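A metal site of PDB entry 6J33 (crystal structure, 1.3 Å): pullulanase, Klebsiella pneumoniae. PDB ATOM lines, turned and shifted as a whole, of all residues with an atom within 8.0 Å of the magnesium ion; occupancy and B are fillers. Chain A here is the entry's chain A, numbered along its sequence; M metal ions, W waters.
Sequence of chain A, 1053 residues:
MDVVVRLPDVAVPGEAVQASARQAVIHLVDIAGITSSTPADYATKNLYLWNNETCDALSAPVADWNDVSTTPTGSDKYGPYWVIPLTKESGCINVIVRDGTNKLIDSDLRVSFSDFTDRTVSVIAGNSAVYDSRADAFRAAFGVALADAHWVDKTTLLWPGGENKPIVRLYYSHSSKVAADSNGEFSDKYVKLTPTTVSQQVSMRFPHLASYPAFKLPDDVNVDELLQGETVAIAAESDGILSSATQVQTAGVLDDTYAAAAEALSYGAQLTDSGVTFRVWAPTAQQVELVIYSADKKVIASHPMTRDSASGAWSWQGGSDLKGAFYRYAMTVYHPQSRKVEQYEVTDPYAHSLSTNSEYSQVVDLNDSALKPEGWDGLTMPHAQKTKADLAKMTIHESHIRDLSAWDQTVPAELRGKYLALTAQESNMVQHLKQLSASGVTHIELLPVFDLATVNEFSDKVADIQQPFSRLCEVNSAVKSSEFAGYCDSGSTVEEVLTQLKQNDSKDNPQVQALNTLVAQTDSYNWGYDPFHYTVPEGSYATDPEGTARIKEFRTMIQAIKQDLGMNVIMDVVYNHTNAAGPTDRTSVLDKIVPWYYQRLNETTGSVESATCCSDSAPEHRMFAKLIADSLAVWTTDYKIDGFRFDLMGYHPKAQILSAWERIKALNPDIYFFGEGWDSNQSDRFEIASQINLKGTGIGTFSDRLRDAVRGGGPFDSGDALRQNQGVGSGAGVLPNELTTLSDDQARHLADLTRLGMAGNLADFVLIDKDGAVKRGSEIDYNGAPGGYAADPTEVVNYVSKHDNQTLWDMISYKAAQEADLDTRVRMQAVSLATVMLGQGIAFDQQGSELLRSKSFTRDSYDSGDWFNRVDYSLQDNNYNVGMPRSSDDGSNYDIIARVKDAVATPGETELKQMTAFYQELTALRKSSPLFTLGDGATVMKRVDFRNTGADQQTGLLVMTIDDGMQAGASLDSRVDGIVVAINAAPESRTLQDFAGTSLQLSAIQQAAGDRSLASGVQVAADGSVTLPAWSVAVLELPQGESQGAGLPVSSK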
ATOM      1  N   SER A 929       3.185  11.349 -11.718  1.00  0.00           N
ATOM      2  CA  SER A 929       4.178  12.377 -11.465  1.00  0.00           C
ATOM      3  C   SER A 929       5.117  11.874 -10.378  1.00  0.00           C
ATOM      4  O   SER A 929       4.650  11.251  -9.415  1.00  0.00           O
ATOM      5  CB  SER A 929       3.526  13.669 -10.984  1.00  0.00           C
ATOM      6  OG  SER A 929       4.513  14.628 -10.648  1.00  0.00           O
ATOM      7  N   LEU A 931       6.099  13.695  -8.197  1.00  0.00           N
ATOM      8  CA  LEU A 931       5.786  14.525  -7.037  1.00  0.00           C
ATOM      9  C   LEU A 931       4.932  13.806  -6.000  1.00  0.00           C
ATOM     10  O   LEU A 931       4.949  14.204  -4.837  1.00  0.00           O
ATOM     11  CB  LEU A 931       5.077  15.801  -7.497  1.00  0.00           C
ATOM     12  CG  LEU A 931       5.954  16.753  -8.330  1.00  0.00           C
ATOM     13  CD1 LEU A 931       5.106  17.871  -8.909  1.00  0.00           C
ATOM     14  CD2 LEU A 931       7.063  17.317  -7.471  1.00  0.00           C
ATOM     15  N   ARG A 943       8.297  20.531   0.124  1.00  0.00           N
ATOM     16  CA  ARG A 943       7.381  20.641  -0.974  1.00  0.00           C
ATOM     17  C   ARG A 943       5.887  20.460  -0.722  1.00  0.00           C
ATOM     18  O   ARG A 943       5.106  20.966  -1.470  1.00  0.00           O
ATOM     19  CB  ARG A 943       7.783  19.646  -2.057  1.00  0.00           C
ATOM     20  CG  ARG A 943       9.148  19.875  -2.677  1.00  0.00           C
ATOM     21  CD  ARG A 943       9.560  18.777  -3.625  1.00  0.00           C
ATOM     22  NE  ARG A 943      10.873  19.024  -4.201  1.00  0.00           N
ATOM     23  CZ  ARG A 943      11.094  19.411  -5.441  1.00  0.00           C
ATOM     24  NH1 ARG A 943      10.117  19.692  -6.251  1.00  0.00           N
ATOM     25  NH2 ARG A 943      12.316  19.567  -5.852  1.00  0.00           N
ATOM     26  N   ASP A 963       4.860  21.191  -4.293  1.00  0.00           N
ATOM     27  CA  ASP A 963       5.595  22.221  -5.013  1.00  0.00           C
ATOM     28  C   ASP A 963       6.639  21.609  -5.944  1.00  0.00           C
ATOM     29  O   ASP A 963       7.397  20.722  -5.555  1.00  0.00           O
ATOM     30  CB  ASP A 963       6.267  23.151  -4.015  1.00  0.00           C
ATOM     31  CG  ASP A 963       6.850  24.403  -4.659  1.00  0.00           C
ATOM     32  OD1 ASP A 963       6.439  24.755  -5.795  1.00  0.00           O
ATOM     33  OD2 ASP A 963       7.717  25.031  -4.020  1.00  0.00           O
ATOM     34  N   ASP A 964       6.668  22.103  -7.189  1.00  0.00           N
ATOM     35  CA  ASP A 964       7.794  21.878  -8.077  1.00  0.00           C
ATOM     36  C   ASP A 964       8.448  23.177  -8.525  1.00  0.00           C
ATOM     37  O   ASP A 964       9.242  23.179  -9.478  1.00  0.00           O
ATOM     38  CB  ASP A 964       7.390  21.027  -9.292  1.00  0.00           C
ATOM     39  CG  ASP A 964       8.548  20.177  -9.819  1.00  0.00           C
ATOM     40  OD1 ASP A 964       9.390  19.726  -9.016  1.00  0.00           O
ATOM     41  OD2 ASP A 964       8.591  19.972 -11.054  1.00  0.00           O
ATOM     42  N   GLY A 965       8.140  24.297  -7.860  1.00  0.00           N
ATOM     43  CA  GLY A 965       8.646  25.584  -8.263  1.00  0.00           C
ATOM     44  C   GLY A 965      10.039  25.888  -7.726  1.00  0.00           C
ATOM     45  O   GLY A 965      10.667  25.087  -7.032  1.00  0.00           O
ATOM     46  N   ALA A 970      15.110  21.849  -7.443  1.00  0.00           N
ATOM     47  CA  ALA A 970      15.030  21.486  -8.846  1.00  0.00           C
ATOM     48  C   ALA A 970      13.609  21.092  -9.211  1.00  0.00           C
ATOM     49  O   ALA A 970      12.815  20.662  -8.361  1.00  0.00           O
ATOM     50  CB  ALA A 970      15.974  20.322  -9.150  1.00  0.00           C
ATOM     51  N   SER A 971      13.268  21.267 -10.482  1.00  0.00           N
ATOM     52  CA  SER A 971      12.047  20.692 -11.010  1.00  0.00           C
ATOM     53  C   SER A 971      12.227  19.186 -11.099  1.00  0.00           C
ATOM     54  O   SER A 971      13.131  18.706 -11.779  1.00  0.00           O
ATOM     55  CB  SER A 971      11.767  21.267 -12.402  1.00  0.00           C
ATOM     56  OG  SER A 971      10.696  20.585 -13.031  1.00  0.00           O
ATOM     57  N   LEU A 972      11.377  18.445 -10.383  1.00  0.00           N
ATOM     58  CA  LEU A 972      11.391  16.992 -10.462  1.00  0.00           C
ATOM     59  C   LEU A 972      10.426  16.459 -11.508  1.00  0.00           C
ATOM     60  O   LEU A 972      10.505  15.270 -11.853  1.00  0.00           O
ATOM     61  CB  LEU A 972      11.054  16.377  -9.103  1.00  0.00           C
ATOM     62  CG  LEU A 972      11.937  16.807  -7.951  1.00  0.00           C
ATOM     63  CD1 LEU A 972      11.386  16.279  -6.638  1.00  0.00           C
ATOM     64  CD2 LEU A 972      13.362  16.317  -8.172  1.00  0.00           C
ATOM     65  N   ASP A 973       9.527  17.293 -12.020  1.00  0.00           N
ATOM     66  CA  ASP A 973       8.582  16.925 -13.061  1.00  0.00           C
ATOM     67  C   ASP A 973       8.631  18.018 -14.118  1.00  0.00           C
ATOM     68  O   ASP A 973       8.267  19.164 -13.852  1.00  0.00           O
ATOM     69  CB  ASP A 973       7.165  16.803 -12.491  1.00  0.00           C
ATOM     70  CG  ASP A 973       6.164  16.241 -13.500  1.00  0.00           C
ATOM     71  OD1 ASP A 973       6.304  16.509 -14.714  1.00  0.00           O
ATOM     72  OD2 ASP A 973       5.240  15.517 -13.074  1.00  0.00           O
ATOM     73  N   SER A 974       9.061  17.653 -15.325  1.00  0.00           N
ATOM     74  CA  SER A 974       9.240  18.640 -16.384  1.00  0.00           C
ATOM     75  C   SER A 974       7.916  19.168 -16.929  1.00  0.00           C
ATOM     76  O   SER A 974       7.914  20.187 -17.626  1.00  0.00           O
ATOM     77  CB  SER A 974      10.059  18.035 -17.531  1.00  0.00           C
ATOM     78  OG  SER A 974       9.379  16.945 -18.110  1.00  0.00           O
ATOM     79  N   ARG A 975       6.798  18.498 -16.647  1.00  0.00           N
ATOM     80  CA  ARG A 975       5.503  18.932 -17.164  1.00  0.00           C
ATOM     81  C   ARG A 975       4.815  19.958 -16.283  1.00  0.00           C
ATOM     82  O   ARG A 975       4.013  20.749 -16.784  1.00  0.00           O
ATOM     83  CB  ARG A 975       4.552  17.736 -17.305  1.00  0.00           C
ATOM     84  CG  ARG A 975       5.078  16.570 -18.107  1.00  0.00           C
ATOM     85  CD  ARG A 975       4.177  15.353 -17.900  1.00  0.00           C
ATOM     86  NE  ARG A 975       4.078  14.996 -16.486  1.00  0.00           N
ATOM     87  CZ  ARG A 975       3.001  15.174 -15.732  1.00  0.00           C
ATOM     88  NH1 ARG A 975       3.033  14.808 -14.455  1.00  0.00           N
ATOM     89  NH2 ARG A 975       1.895  15.701 -16.233  1.00  0.00           N
ATOM     90  N   VAL A 976       5.087  19.952 -14.986  1.00  0.00           N
ATOM     91  CA  VAL A 976       4.335  20.764 -14.033  1.00  0.00           C
ATOM     92  C   VAL A 976       5.269  21.520 -13.090  1.00  0.00           C
ATOM     93  O   VAL A 976       6.377  21.075 -12.783  1.00  0.00           O
ATOM     94  CB  VAL A 976       3.327  19.928 -13.209  1.00  0.00           C
ATOM     95  CG1 VAL A 976       2.355  19.182 -14.126  1.00  0.00           C
ATOM     96  CG2 VAL A 976       4.040  18.962 -12.278  1.00  0.00           C
ATOM     97  N   ASP A 977       4.789  22.676 -12.625  1.00  0.00           N
ATOM     98  CA  ASP A 977       5.406  23.426 -11.545  1.00  0.00           C
ATOM     99  C   ASP A 977       4.779  23.119 -10.189  1.00  0.00           C
ATOM    100  O   ASP A 977       5.241  23.648  -9.166  1.00  0.00           O
ATOM    101  CB  ASP A 977       5.325  24.926 -11.817  1.00  0.00           C
ATOM    102  CG  ASP A 977       6.227  25.367 -12.968  1.00  0.00           C
ATOM    103  OD1 ASP A 977       7.378  24.896 -13.038  1.00  0.00           O
ATOM    104  OD2 ASP A 977       5.780  26.195 -13.775  1.00  0.00           O
ATOM    105  N   GLY A 978       3.728  22.315 -10.156  1.00  0.00           N
ATOM    106  CA  GLY A 978       3.108  21.950  -8.898  1.00  0.00           C
ATOM    107  C   GLY A 978       1.849  21.153  -9.149  1.00  0.00           C
ATOM    108  O   GLY A 978       1.309  21.150 -10.263  1.00  0.00           O
ATOM    109  N   LEU A1038      -0.200  22.674 -12.307  1.00  0.00           N
ATOM    110  CA  LEU A1038       0.295  23.937 -12.841  1.00  0.00           C
ATOM    111  C   LEU A1038       1.234  23.580 -13.995  1.00  0.00           C
ATOM    112  O   LEU A1038       2.332  23.085 -13.748  1.00  0.00           O
ATOM    113  CB  LEU A1038       1.066  24.704 -11.775  1.00  0.00           C
ATOM    114  CG  LEU A1038       0.335  25.399 -10.634  1.00  0.00           C
ATOM    115  CD1 LEU A1038       1.346  26.053  -9.709  1.00  0.00           C
ATOM    116  CD2 LEU A1038      -0.632  26.451 -11.172  1.00  0.00           C
ATOM    117  N   PRO A1039       0.841  23.814 -15.244  1.00  0.00           N
ATOM    118  CA  PRO A1039       1.694  23.390 -16.364  1.00  0.00           C
ATOM    119  C   PRO A1039       2.994  24.169 -16.380  1.00  0.00           C
ATOM    120  O   PRO A1039       3.021  25.376 -16.106  1.00  0.00           O
ATOM    121  CB  PRO A1039       0.840  23.709 -17.605  1.00  0.00           C
ATOM    122  CG  PRO A1039      -0.522  23.989 -17.097  1.00  0.00           C
ATOM    123  CD  PRO A1039      -0.389  24.483 -15.704  1.00  0.00           C
ATOM    124  N   GLN A1040       4.080  23.480 -16.699  1.00  0.00           N
ATOM    125  CA  GLN A1040       5.393  24.086 -16.696  1.00  0.00           C
ATOM    126  C   GLN A1040       5.675  24.682 -18.070  1.00  0.00           C
ATOM    127  O   GLN A1040       5.501  24.013 -19.098  1.00  0.00           O
ATOM    128  CB  GLN A1040       6.473  23.057 -16.328  1.00  0.00           C
ATOM    129  CG  GLN A1040       7.852  23.658 -16.117  1.00  0.00           C
ATOM    130  CD  GLN A1040       8.814  22.687 -15.461  1.00  0.00           C
ATOM    131  OE1 GLN A1040       8.412  21.865 -14.624  1.00  0.00           O
ATOM    132  NE2 GLN A1040      10.090  22.759 -15.822  1.00  0.00           N
ATOM    133  N   GLY A1041       6.076  25.955 -18.081  1.00  0.00           N
ATOM    134  CA  GLY A1041       6.353  26.654 -19.319  1.00  0.00           C
ATOM    135  C   GLY A1041       7.771  26.465 -19.835  1.00  0.00           C
ATOM    136  O   GLY A1041       8.334  25.380 -19.721  1.00  0.00           O
ATOM    137  N   SER A1043      10.551  27.694 -18.717  1.00  0.00           N
ATOM    138  CA  SER A1043      11.455  27.455 -17.605  1.00  0.00           C
ATOM    139  C   SER A1043      10.643  27.165 -16.361  1.00  0.00           C
ATOM    140  O   SER A1043       9.425  27.392 -16.318  1.00  0.00           O
ATOM    141  CB  SER A1043      12.399  28.644 -17.374  1.00  0.00           C
ATOM    142  OG  SER A1043      13.217  28.882 -18.505  1.00  0.00           O
ATOM    143  N   GLN A1044      11.320  26.637 -15.331  1.00  0.00           N
ATOM    144  CA  GLN A1044      10.666  26.313 -14.078  1.00  0.00           C
ATOM    145  C   GLN A1044       9.999  27.555 -13.496  1.00  0.00           C
ATOM    146  O   GLN A1044      10.593  28.648 -13.489  1.00  0.00           O
ATOM    147  CB  GLN A1044      11.687  25.776 -13.082  1.00  0.00           C
ATOM    148  CG  GLN A1044      11.160  25.536 -11.669  1.00  0.00           C
ATOM    149  CD  GLN A1044      12.262  25.117 -10.699  1.00  0.00           C
ATOM    150  OE1 GLN A1044      13.396  25.585 -10.800  1.00  0.00           O
ATOM    151  NE2 GLN A1044      11.931  24.242  -9.762  1.00  0.00           N
ATOM    152  N   GLY A1045       8.760  27.398 -13.017  1.00  0.00           N
ATOM    153  CA  GLY A1045       7.951  28.500 -12.575  1.00  0.00           C
ATOM    154  C   GLY A1045       7.916  28.665 -11.065  1.00  0.00           C
ATOM    155  O   GLY A1045       8.696  28.065 -10.314  1.00  0.00           O
HETATM  156 MG    MG M   1       8.504  20.930 -12.904  1.00  0.00          MG
HETATM  157  O   HOH W   1       8.778  22.837 -12.059  1.00  0.00           O
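Water W1 bridges O of Asp 964 and OD1 of Asp 977.
The backbone carbonyl oxygen of Arg 975 sits at hydrogen-bond distance from the backbone NH of Gln 1040 (2.7 Å).
The side-chain carboxylate (OD2) of Asp 973 is in salt-bridge range of the guanidinium group (NH1) of Arg 975 (2.7 Å).
The side-chain hydroxyl (OG) of Ser 929 lies within hydrogen-bond range of the side-chain carboxylate (OD2) of Asp 973 (2.7 Å).
N of Asp 964 sits at hydrogen-bond distance from O of Asp 977, 2.9 Å away.
The side-chain carboxylate (OD1) of Asp 964 is in hydrogen-bond range of the backbone NH (N) of Leu 972 (2.7 Å).
The side-chain amide nitrogen of Gln 1044 lies within hydrogen-bond range of the backbone carbonyl oxygen of Asp 964, at 2.9 Å.
The side-chain carboxylate of Asp 964 lies within salt-bridge range of the guanidinium group of Arg 943, 2.9 Å away.
N of Ser 971 sits close to NE2 of Gln 1044 (3.3 Å).
The magnesium ion is bound by the side-chain amide oxygen (OE1) of Gln 1040, at 2.0 Å.
O of Asp 973 binds the magnesium ion (2.0 Å).
The magnesium ion is bound by the side-chain carboxylate (OD2) of Asp 964, 2.1 Å away.
The magnesium ion is bound by water W1, at 2.1 Å.
O of Val 976 binds the magnesium ion, 2.1 Å away.
OG of Ser 971 binds the magnesium ion.
Within 4 Å of the magnesium ion: Asp 964, Ser 971, Asp 973, Val 976 and Gln 1040.
The nearest printed residue that does not touch the magnesium ion is Ser 974 (4.1 Å).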
